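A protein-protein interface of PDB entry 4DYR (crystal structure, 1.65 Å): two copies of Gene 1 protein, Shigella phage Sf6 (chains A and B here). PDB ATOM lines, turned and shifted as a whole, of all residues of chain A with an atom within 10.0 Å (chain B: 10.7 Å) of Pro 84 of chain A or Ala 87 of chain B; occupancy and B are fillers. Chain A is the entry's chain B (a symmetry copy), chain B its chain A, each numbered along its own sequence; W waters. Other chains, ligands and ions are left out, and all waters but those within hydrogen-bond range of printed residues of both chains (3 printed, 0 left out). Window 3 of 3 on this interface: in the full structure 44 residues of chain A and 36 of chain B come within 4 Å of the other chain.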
ATOM      1  N   ILE A  78      -2.891  -7.161   5.709  1.00  0.00           N
ATOM      2  CA  ILE A  78      -2.145  -6.075   6.340  1.00  0.00           C
ATOM      3  C   ILE A  78      -1.809  -4.981   5.330  1.00  0.00           C
ATOM      4  O   ILE A  78      -1.929  -3.790   5.624  1.00  0.00           O
ATOM      5  CB  ILE A  78      -0.862  -6.592   7.010  1.00  0.00           C
ATOM      6  CG1 ILE A  78      -1.240  -7.568   8.133  1.00  0.00           C
ATOM      7  CG2 ILE A  78      -0.023  -5.429   7.547  1.00  0.00           C
ATOM      8  CD1 ILE A  78      -0.059  -8.245   8.792  1.00  0.00           C
ATOM      9  N   ALA A  79      -1.396  -5.397   4.138  1.00  0.00           N
ATOM     10  CA  ALA A  79      -1.024  -4.444   3.096  1.00  0.00           C
ATOM     11  C   ALA A  79      -2.249  -3.713   2.573  1.00  0.00           C
ATOM     12  O   ALA A  79      -2.271  -2.484   2.494  1.00  0.00           O
ATOM     13  CB  ALA A  79      -0.318  -5.161   1.949  1.00  0.00           C
ATOM     14  N   ASP A  80      -3.278  -4.480   2.238  1.00  0.00           N
ATOM     15  CA  ASP A  80      -4.436  -3.927   1.543  1.00  0.00           C
ATOM     16  C   ASP A  80      -5.251  -3.014   2.456  1.00  0.00           C
ATOM     17  O   ASP A  80      -5.912  -2.087   1.986  1.00  0.00           O
ATOM     18  CB  ASP A  80      -5.337  -5.050   1.028  1.00  0.00           C
ATOM     19  CG  ASP A  80      -4.730  -5.811  -0.133  1.00  0.00           C
ATOM     20  OD1 ASP A  80      -3.730  -5.339  -0.724  1.00  0.00           O
ATOM     21  OD2 ASP A  80      -5.289  -6.872  -0.475  1.00  0.00           O
ATOM     22  N   ASN A  81      -5.220  -3.289   3.753  1.00  0.00           N
ATOM     23  CA  ASN A  81      -6.050  -2.540   4.687  1.00  0.00           C
ATOM     24  C   ASN A  81      -5.284  -1.454   5.420  1.00  0.00           C
ATOM     25  O   ASN A  81      -5.820  -0.809   6.311  1.00  0.00           O
ATOM     26  CB  ASN A  81      -6.735  -3.482   5.685  1.00  0.00           C
ATOM     27  CG  ASN A  81      -7.699  -4.449   5.011  1.00  0.00           C
ATOM     28  OD1 ASN A  81      -8.228  -4.172   3.943  1.00  0.00           O
ATOM     29  ND2 ASN A  81      -7.925  -5.590   5.642  1.00  0.00           N
ATOM     30  N   ALA A  82      -4.021  -1.248   5.054  1.00  0.00           N
ATOM     31  CA  ALA A  82      -3.213  -0.260   5.755  1.00  0.00           C
ATOM     32  C   ALA A  82      -3.880   1.119   5.699  1.00  0.00           C
ATOM     33  O   ALA A  82      -4.353   1.543   4.651  1.00  0.00           O
ATOM     34  CB  ALA A  82      -1.807  -0.192   5.144  1.00  0.00           C
ATOM     35  N   ILE A  83      -3.917   1.808   6.836  1.00  0.00           N
ATOM     36  CA  ILE A  83      -4.363   3.195   6.865  1.00  0.00           C
ATOM     37  C   ILE A  83      -3.384   4.023   6.040  1.00  0.00           C
ATOM     38  O   ILE A  83      -2.177   3.948   6.267  1.00  0.00           O
ATOM     39  CB  ILE A  83      -4.379   3.745   8.305  1.00  0.00           C
ATOM     40  CG1 ILE A  83      -5.363   2.958   9.173  1.00  0.00           C
ATOM     41  CG2 ILE A  83      -4.712   5.233   8.308  1.00  0.00           C
ATOM     42  CD1 ILE A  83      -5.230   3.246  10.656  1.00  0.00           C
ATOM     43  N   PRO A  84      -3.898   4.806   5.071  1.00  0.00           N
ATOM     44  CA  PRO A  84      -3.040   5.592   4.175  1.00  0.00           C
ATOM     45  C   PRO A  84      -2.488   6.834   4.870  1.00  0.00           C
ATOM     46  O   PRO A  84      -2.776   7.972   4.496  1.00  0.00           O
ATOM     47  CB  PRO A  84      -3.982   5.968   3.028  1.00  0.00           C
ATOM     48  CG  PRO A  84      -5.323   5.992   3.649  1.00  0.00           C
ATOM     49  CD  PRO A  84      -5.321   4.920   4.706  1.00  0.00           C
ATOM     50  N   ASP A  85      -1.707   6.580   5.909  1.00  0.00           N
ATOM     51  CA  ASP A  85      -0.972   7.602   6.629  1.00  0.00           C
ATOM     52  C   ASP A  85       0.486   7.162   6.648  1.00  0.00           C
ATOM     53  O   ASP A  85       0.772   5.969   6.750  1.00  0.00           O
ATOM     54  CB  ASP A  85      -1.524   7.728   8.047  1.00  0.00           C
ATOM     55  CG  ASP A  85      -0.528   8.329   9.009  1.00  0.00           C
ATOM     56  OD1 ASP A  85      -0.430   9.575   9.061  1.00  0.00           O
ATOM     57  OD2 ASP A  85       0.151   7.551   9.716  1.00  0.00           O
ATOM     58  N   ALA A  86       1.410   8.109   6.533  1.00  0.00           N
ATOM     59  CA  ALA A  86       2.822   7.759   6.345  1.00  0.00           C
ATOM     60  C   ALA A  86       3.333   6.762   7.387  1.00  0.00           C
ATOM     61  O   ALA A  86       3.919   5.733   7.038  1.00  0.00           O
ATOM     62  CB  ALA A  86       3.695   9.009   6.320  1.00  0.00           C
ATOM     63  N   ALA A  87       3.111   7.067   8.660  1.00  0.00           N
ATOM     64  CA  ALA A  87       3.578   6.207   9.747  1.00  0.00           C
ATOM     65  C   ALA A  87       2.870   4.848   9.781  1.00  0.00           C
ATOM     66  O   ALA A  87       3.505   3.816  10.042  1.00  0.00           O
ATOM     67  CB  ALA A  87       3.430   6.917  11.098  1.00  0.00           C
ATOM     68  N   GLU A  88       1.562   4.849   9.538  1.00  0.00           N
ATOM     69  CA  GLU A  88       0.786   3.611   9.531  1.00  0.00           C
ATOM     70  C   GLU A  88       1.202   2.703   8.379  1.00  0.00           C
ATOM     71  O   GLU A  88       1.243   1.481   8.530  1.00  0.00           O
ATOM     72  CB  GLU A  88      -0.721   3.894   9.452  1.00  0.00           C
ATOM     73  CG  GLU A  88      -1.314   4.588  10.687  1.00  0.00           C
ATOM     74  CD  GLU A  88      -1.451   3.677  11.904  1.00  0.00           C
ATOM     75  OE1 GLU A  88      -1.049   2.494  11.844  1.00  0.00           O
ATOM     76  OE2 GLU A  88      -1.963   4.153  12.939  1.00  0.00           O
ATOM     77  N   VAL A  89       1.485   3.292   7.222  1.00  0.00           N
ATOM     78  CA  VAL A  89       1.974   2.492   6.101  1.00  0.00           C
ATOM     79  C   VAL A  89       3.358   1.912   6.390  1.00  0.00           C
ATOM     80  O   VAL A  89       3.617   0.746   6.092  1.00  0.00           O
ATOM     81  CB  VAL A  89       1.998   3.293   4.793  1.00  0.00           C
ATOM     82  CG1 VAL A  89       2.684   2.492   3.683  1.00  0.00           C
ATOM     83  CG2 VAL A  89       0.590   3.666   4.394  1.00  0.00           C
ATOM     84  N   ALA A  90       4.239   2.713   6.991  1.00  0.00           N
ATOM     85  CA  ALA A  90       5.552   2.211   7.375  1.00  0.00           C
ATOM     86  C   ALA A  90       5.425   1.059   8.378  1.00  0.00           C
ATOM     87  O   ALA A  90       6.157   0.065   8.289  1.00  0.00           O
ATOM     88  CB  ALA A  90       6.435   3.346   7.938  1.00  0.00           C
ATOM     89  N   ALA A  92       2.787  -0.974   8.675  1.00  0.00           N
ATOM     90  CA  ALA A  92       2.251  -2.116   7.937  1.00  0.00           C
ATOM     91  C   ALA A  92       3.359  -2.813   7.159  1.00  0.00           C
ATOM     92  O   ALA A  92       3.438  -4.038   7.148  1.00  0.00           O
ATOM     93  CB  ALA A  92       1.125  -1.686   7.002  1.00  0.00           C
ATOM     94  N   ARG A  93       4.202  -2.022   6.501  1.00  0.00           N
ATOM     95  CA  ARG A  93       5.372  -2.561   5.796  1.00  0.00           C
ATOM     96  C   ARG A  93       6.278  -3.363   6.728  1.00  0.00           C
ATOM     97  O   ARG A  93       6.726  -4.458   6.393  1.00  0.00           O
ATOM     98  CB  ARG A  93       6.170  -1.433   5.125  1.00  0.00           C
ATOM     99  CG  ARG A  93       7.343  -1.929   4.274  1.00  0.00           C
ATOM    100  CD  ARG A  93       8.108  -0.766   3.652  1.00  0.00           C
ATOM    101  NE  ARG A  93       9.443  -1.175   3.229  1.00  0.00           N
ATOM    102  CZ  ARG A  93      10.426  -0.334   2.921  1.00  0.00           C
ATOM    103  NH1 ARG A  93      10.227   0.978   2.985  1.00  0.00           N
ATOM    104  NH2 ARG A  93      11.610  -0.804   2.552  1.00  0.00           N
ATOM    105  N   ILE B  78      -2.721  -1.838  -9.659  1.00  0.00           N
ATOM    106  CA  ILE B  78      -2.438  -1.177  -8.394  1.00  0.00           C
ATOM    107  C   ILE B  78      -1.383  -0.100  -8.602  1.00  0.00           C
ATOM    108  O   ILE B  78      -1.501   0.998  -8.066  1.00  0.00           O
ATOM    109  CB  ILE B  78      -1.982  -2.171  -7.315  1.00  0.00           C
ATOM    110  CG1 ILE B  78      -3.125  -3.140  -7.007  1.00  0.00           C
ATOM    111  CG2 ILE B  78      -1.571  -1.430  -6.032  1.00  0.00           C
ATOM    112  CD1 ILE B  78      -2.721  -4.326  -6.149  1.00  0.00           C
ATOM    113  N   ALA B  82      -2.481   4.079  -8.755  1.00  0.00           N
ATOM    114  CA  ALA B  82      -2.176   4.611  -7.433  1.00  0.00           C
ATOM    115  C   ALA B  82      -2.521   6.100  -7.354  1.00  0.00           C
ATOM    116  O   ALA B  82      -2.205   6.864  -8.258  1.00  0.00           O
ATOM    117  CB  ALA B  82      -0.712   4.391  -7.102  1.00  0.00           C
ATOM    118  N   ILE B  83      -3.171   6.506  -6.270  1.00  0.00           N
ATOM    119  CA  ILE B  83      -3.419   7.923  -6.029  1.00  0.00           C
ATOM    120  C   ILE B  83      -2.091   8.645  -5.772  1.00  0.00           C
ATOM    121  O   ILE B  83      -1.281   8.203  -4.945  1.00  0.00           O
ATOM    122  CB  ILE B  83      -4.387   8.120  -4.841  1.00  0.00           C
ATOM    123  CG1 ILE B  83      -5.752   7.492  -5.162  1.00  0.00           C
ATOM    124  CG2 ILE B  83      -4.520   9.593  -4.506  1.00  0.00           C
ATOM    125  CD1 ILE B  83      -6.588   7.161  -3.946  1.00  0.00           C
ATOM    126  N   PRO B  84      -1.845   9.750  -6.496  1.00  0.00           N
ATOM    127  CA  PRO B  84      -0.547  10.434  -6.432  1.00  0.00           C
ATOM    128  C   PRO B  84      -0.385  11.282  -5.170  1.00  0.00           C
ATOM    129  O   PRO B  84      -0.214  12.503  -5.219  1.00  0.00           O
ATOM    130  CB  PRO B  84      -0.548  11.305  -7.693  1.00  0.00           C
ATOM    131  CG  PRO B  84      -1.970  11.584  -7.946  1.00  0.00           C
ATOM    132  CD  PRO B  84      -2.742  10.362  -7.491  1.00  0.00           C
ATOM    133  N   ASP B  85      -0.449  10.599  -4.036  1.00  0.00           N
ATOM    134  CA  ASP B  85      -0.223  11.178  -2.726  1.00  0.00           C
ATOM    135  C   ASP B  85       0.816  10.292  -2.039  1.00  0.00           C
ATOM    136  O   ASP B  85       0.817   9.081  -2.237  1.00  0.00           O
ATOM    137  CB  ASP B  85      -1.536  11.189  -1.948  1.00  0.00           C
ATOM    138  CG  ASP B  85      -1.332  11.115  -0.454  1.00  0.00           C
ATOM    139  OD1 ASP B  85      -1.191  12.181   0.182  1.00  0.00           O
ATOM    140  OD2 ASP B  85      -1.322   9.986   0.085  1.00  0.00           O
ATOM    141  N   ALA B  86       1.705  10.886  -1.251  1.00  0.00           N
ATOM    142  CA  ALA B  86       2.843  10.145  -0.709  1.00  0.00           C
ATOM    143  C   ALA B  86       2.430   8.840  -0.035  1.00  0.00           C
ATOM    144  O   ALA B  86       2.939   7.769  -0.374  1.00  0.00           O
ATOM    145  CB  ALA B  86       3.651  11.015   0.254  1.00  0.00           C
ATOM    146  N   ALA B  87       1.506   8.926   0.916  1.00  0.00           N
ATOM    147  CA  ALA B  87       1.109   7.748   1.681  1.00  0.00           C
ATOM    148  C   ALA B  87       0.361   6.716   0.834  1.00  0.00           C
ATOM    149  O   ALA B  87       0.541   5.510   1.025  1.00  0.00           O
ATOM    150  CB  ALA B  87       0.276   8.147   2.890  1.00  0.00           C
ATOM    151  N   GLU B  88      -0.496   7.184  -0.069  1.00  0.00           N
ATOM    152  CA  GLU B  88      -1.207   6.276  -0.966  1.00  0.00           C
ATOM    153  C   GLU B  88      -0.237   5.558  -1.909  1.00  0.00           C
ATOM    154  O   GLU B  88      -0.406   4.372  -2.173  1.00  0.00           O
ATOM    155  CB  GLU B  88      -2.291   7.002  -1.771  1.00  0.00           C
ATOM    156  CG  GLU B  88      -3.457   7.528  -0.936  1.00  0.00           C
ATOM    157  CD  GLU B  88      -4.422   6.444  -0.461  1.00  0.00           C
ATOM    158  OE1 GLU B  88      -4.165   5.238  -0.671  1.00  0.00           O
ATOM    159  OE2 GLU B  88      -5.454   6.802   0.139  1.00  0.00           O
ATOM    160  N   VAL B  89       0.775   6.263  -2.411  1.00  0.00           N
ATOM    161  CA  VAL B  89       1.776   5.611  -3.255  1.00  0.00           C
ATOM    162  C   VAL B  89       2.584   4.591  -2.441  1.00  0.00           C
ATOM    163  O   VAL B  89       2.849   3.478  -2.919  1.00  0.00           O
ATOM    164  CB  VAL B  89       2.727   6.620  -3.939  1.00  0.00           C
ATOM    165  CG1 VAL B  89       3.817   5.879  -4.720  1.00  0.00           C
ATOM    166  CG2 VAL B  89       1.942   7.549  -4.857  1.00  0.00           C
ATOM    167  N   ALA B  90       2.967   4.960  -1.212  1.00  0.00           N
ATOM    168  CA  ALA B  90       3.649   4.023  -0.316  1.00  0.00           C
ATOM    169  C   ALA B  90       2.799   2.776  -0.050  1.00  0.00           C
ATOM    170  O   ALA B  90       3.308   1.652  -0.028  1.00  0.00           O
ATOM    171  CB  ALA B  90       4.047   4.705   1.007  1.00  0.00           C
ATOM    172  N   LYS B  91       1.497   2.970   0.143  1.00  0.00           N
ATOM    173  CA  LYS B  91       0.604   1.832   0.346  1.00  0.00           C
ATOM    174  C   LYS B  91       0.518   0.960  -0.907  1.00  0.00           C
ATOM    175  O   LYS B  91       0.606  -0.267  -0.822  1.00  0.00           O
ATOM    176  CB  LYS B  91      -0.793   2.303   0.758  1.00  0.00           C
ATOM    177  CG  LYS B  91      -1.786   1.171   0.876  1.00  0.00           C
ATOM    178  CD  LYS B  91      -3.124   1.660   1.445  1.00  0.00           C
ATOM    179  CE  LYS B  91      -4.144   0.535   1.443  1.00  0.00           C
ATOM    180  NZ  LYS B  91      -5.438   0.956   2.092  1.00  0.00           N
ATOM    181  N   ALA B  92       0.378   1.603  -2.065  1.00  0.00           N
ATOM    182  CA  ALA B  92       0.342   0.882  -3.339  1.00  0.00           C
ATOM    183  C   ALA B  92       1.617   0.064  -3.504  1.00  0.00           C
ATOM    184  O   ALA B  92       1.568  -1.092  -3.928  1.00  0.00           O
ATOM    185  CB  ALA B  92       0.172   1.841  -4.492  1.00  0.00           C
ATOM    186  N   ARG B  93       2.754   0.666  -3.170  1.00  0.00           N
ATOM    187  CA  ARG B  93       4.021  -0.049  -3.273  1.00  0.00           C
ATOM    188  C   ARG B  93       4.033  -1.267  -2.353  1.00  0.00           C
ATOM    189  O   ARG B  93       4.460  -2.354  -2.749  1.00  0.00           O
ATOM    190  CB  ARG B  93       5.189   0.878  -2.943  1.00  0.00           C
ATOM    191  CG  ARG B  93       6.543   0.228  -3.108  1.00  0.00           C
ATOM    192  CD  ARG B  93       7.638   1.252  -2.839  1.00  0.00           C
ATOM    193  NE  ARG B  93       8.966   0.650  -2.856  1.00  0.00           N
ATOM    194  CZ  ARG B  93      10.037   1.189  -2.282  1.00  0.00           C
ATOM    195  NH1 ARG B  93       9.936   2.345  -1.636  1.00  0.00           N
ATOM    196  NH2 ARG B  93      11.209   0.572  -2.346  1.00  0.00           N
ATOM    197  N   LEU B  94       3.544  -1.105  -1.125  1.00  0.00           N
ATOM    198  CA  LEU B  94       3.473  -2.248  -0.213  1.00  0.00           C
ATOM    199  C   LEU B  94       2.540  -3.349  -0.756  1.00  0.00           C
ATOM    200  O   LEU B  94       2.855  -4.533  -0.682  1.00  0.00           O
ATOM    201  CB  LEU B  94       3.040  -1.799   1.189  1.00  0.00           C
ATOM    202  CG  LEU B  94       2.825  -2.930   2.200  1.00  0.00           C
ATOM    203  CD1 LEU B  94       4.115  -3.728   2.444  1.00  0.00           C
ATOM    204  CD2 LEU B  94       2.309  -2.336   3.510  1.00  0.00           C
ATOM    205  N   ARG B  95       1.409  -2.945  -1.329  1.00  0.00           N
ATOM    206  CA  ARG B  95       0.463  -3.904  -1.887  1.00  0.00           C
ATOM    207  C   ARG B  95       1.095  -4.675  -3.039  1.00  0.00           C
ATOM    208  O   ARG B  95       0.946  -5.896  -3.139  1.00  0.00           O
ATOM    209  CB  ARG B  95      -0.803  -3.186  -2.355  1.00  0.00           C
ATOM    210  CG  ARG B  95      -1.622  -2.633  -1.206  1.00  0.00           C
ATOM    211  CD  ARG B  95      -2.869  -1.985  -1.765  1.00  0.00           C
ATOM    212  NE  ARG B  95      -3.794  -2.988  -2.286  1.00  0.00           N
ATOM    213  CZ  ARG B  95      -4.699  -2.757  -3.230  1.00  0.00           C
ATOM    214  NH1 ARG B  95      -4.779  -1.561  -3.805  1.00  0.00           N
ATOM    215  NH2 ARG B  95      -5.505  -3.737  -3.624  1.00  0.00           N
HETATM  216  O   HOH W   1      -2.806   9.893   2.368  1.00  0.00           O
HETATM  217  O   HOH W   2      -6.378  -1.713  -0.732  1.00  0.00           O
HETATM  218  O   HOH W   3      -8.130   0.087   2.082  1.00  0.00           O
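Among the printed residues, pairs that only touch across the chains: Ala 79 of chain A with Lys 91 of chain B, Ala 79 of chain A with Leu 94 of chain B, Ala 79 of chain A with Arg 95 of chain B, Pro 84 of chain A with Ala 87 of chain B, Pro 84 of chain A with Glu 88 of chain B, Asp 85 of chain A with Ala 87 of chain B, Ala 86 of chain A with Ala 87 of chain B, Val 89 of chain A with Ala 87 of chain B, Val 89 of chain A with Ala 90 of chain B, Val 89 of chain A with Lys 91 of chain B, Ala 92 of chain A with Leu 94 of chain B and Arg 93 of chain A with Leu 94 of chain B.
Pro 84 of chain A touches two residues of chain B.
Ala 87 of chain B touches just these residues of chain A: Pro 84, Asp 85, Ala 86 and Val 89.
Of the printed residues of chain B, Ala 82 of chain A touches Lys 91 (2.8 Å).
Ile 83 of chain A touches none of the printed residues of chain B.
Ala 86 of chain A touches just one residue of chain B: Ala 87 (3.8 Å).
No residue of chain A comes within 4 Å of Ala 86 of chain B.
Of chain A, only Pro 84 comes within 4 Å of Glu 88 of chain B.
Ala 90 of chain B touches just one residue of chain A: Val 89.
Printed residues of chain B within 4 Å of Ala 92 of chain A: Leu 94.
Printed residues of chain B within 4 Å of Val 89 of chain A: Ala 87 (3.8 Å), Ala 90 (3.7 Å) and Lys 91 (3.8 Å).
Of the printed residues of chain B, Asp 80 of chain A touches Lys 91 (3.1 Å) and Arg 95 (2.8 Å).
Of the printed residues of chain B, Ala 79 of chain A touches Lys 91, Leu 94 and Arg 95.
Pro 84 of chain A touches Ala 87 of chain B, but with the chains exchanged Ala 87 of chain A does not touch Pro 84 of chain B (14.9 Å).
Pro 84 of chain A touches Glu 88 of chain B, but with the chains exchanged Glu 88 of chain A does not touch Pro 84 of chain B (16.1 Å).
Ala 86 of chain A touches Ala 87 of chain B, but with the chains exchanged Ala 87 of chain A does not touch Ala 86 of chain B (8.9 Å).
Val 89 of chain A touches Ala 87 of chain B, but with the chains exchanged Ala 87 of chain A does not touch Val 89 of chain B (11.3 Å).
12 positions are printed for both chains.
Of the 15 pairs that touch across the chains among the printed residues, none has its exchanged pair printed and touching as well.
The side-chain carboxylate (OD2) of Asp 85 of chain B sits at hydrogen-bond distance from the backbone NH (N) of Ala 87 of chain B (3.1 Å).
OD2 of Asp 85 of chain B lies within hydrogen-bond range of N of Glu 88 of chain B (2.9 Å).
The backbone NH (N) of Ala 87 of chain A is in hydrogen-bond range of the side-chain carboxylate (OD2) of Asp 85 of chain A (3.2 Å).
The backbone NH (N) of Glu 88 of chain A sits at hydrogen-bond distance from the side-chain carboxylate (OD2) of Asp 85 of chain A, 3.1 Å away.
Water W1 lies within hydrogen-bond range of the side-chain carboxylate of Asp 85 of chain B (2.7 Å) and the backbone carbonyl oxygen of Pro 84 of chain A (2.9 Å).
Water W2 lies within hydrogen-bond range of the backbone carbonyl oxygen (O) of Asp 80 of chain A and the guanidinium group (NE) of Arg 95 of chain B.
Water W3 bridges the side-chain amino group (NZ) of Lys 91 of chain B and the backbone carbonyl oxygen (O) of Asp 80 of chain A.
The backbone carbonyl oxygen of Asp 80 of chain A lies within hydrogen-bond range of the side-chain amino group of Lys 91 of chain B (3.1 Å).
The backbone carbonyl oxygen (O) of Ala 82 of chain A lies within hydrogen-bond range of the side-chain amino group (NZ) of Lys 91 of chain B.
NE of Arg 95 of chain B is in salt-bridge range of OD1 of Asp 80 of chain A (2.8 Å).
Of the 15 printed residues of chain B, 6 touch a printed residue of chain A.
Hydrophobic or aromatic side chains of chain B that line the printed part of chain A: Ala 87, Ala 90 and Leu 94.
Of the 15 printed residues of chain A, 9 touch a printed residue of chain B.
Hydrophobic or aromatic side chains of chain A within 4 Å of the printed part of chain B: Ala 79, Pro 84, Val 89 and Ala 92.
Among the printed residues, 15 pairs touch across the chains.
Among the printed residues, Asp or Glu carboxylates within 4 Å of a Lys or Arg side-chain nitrogen of the other chain: Asp 80 of chain A with Arg 95 of chain B (2.8 Å).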
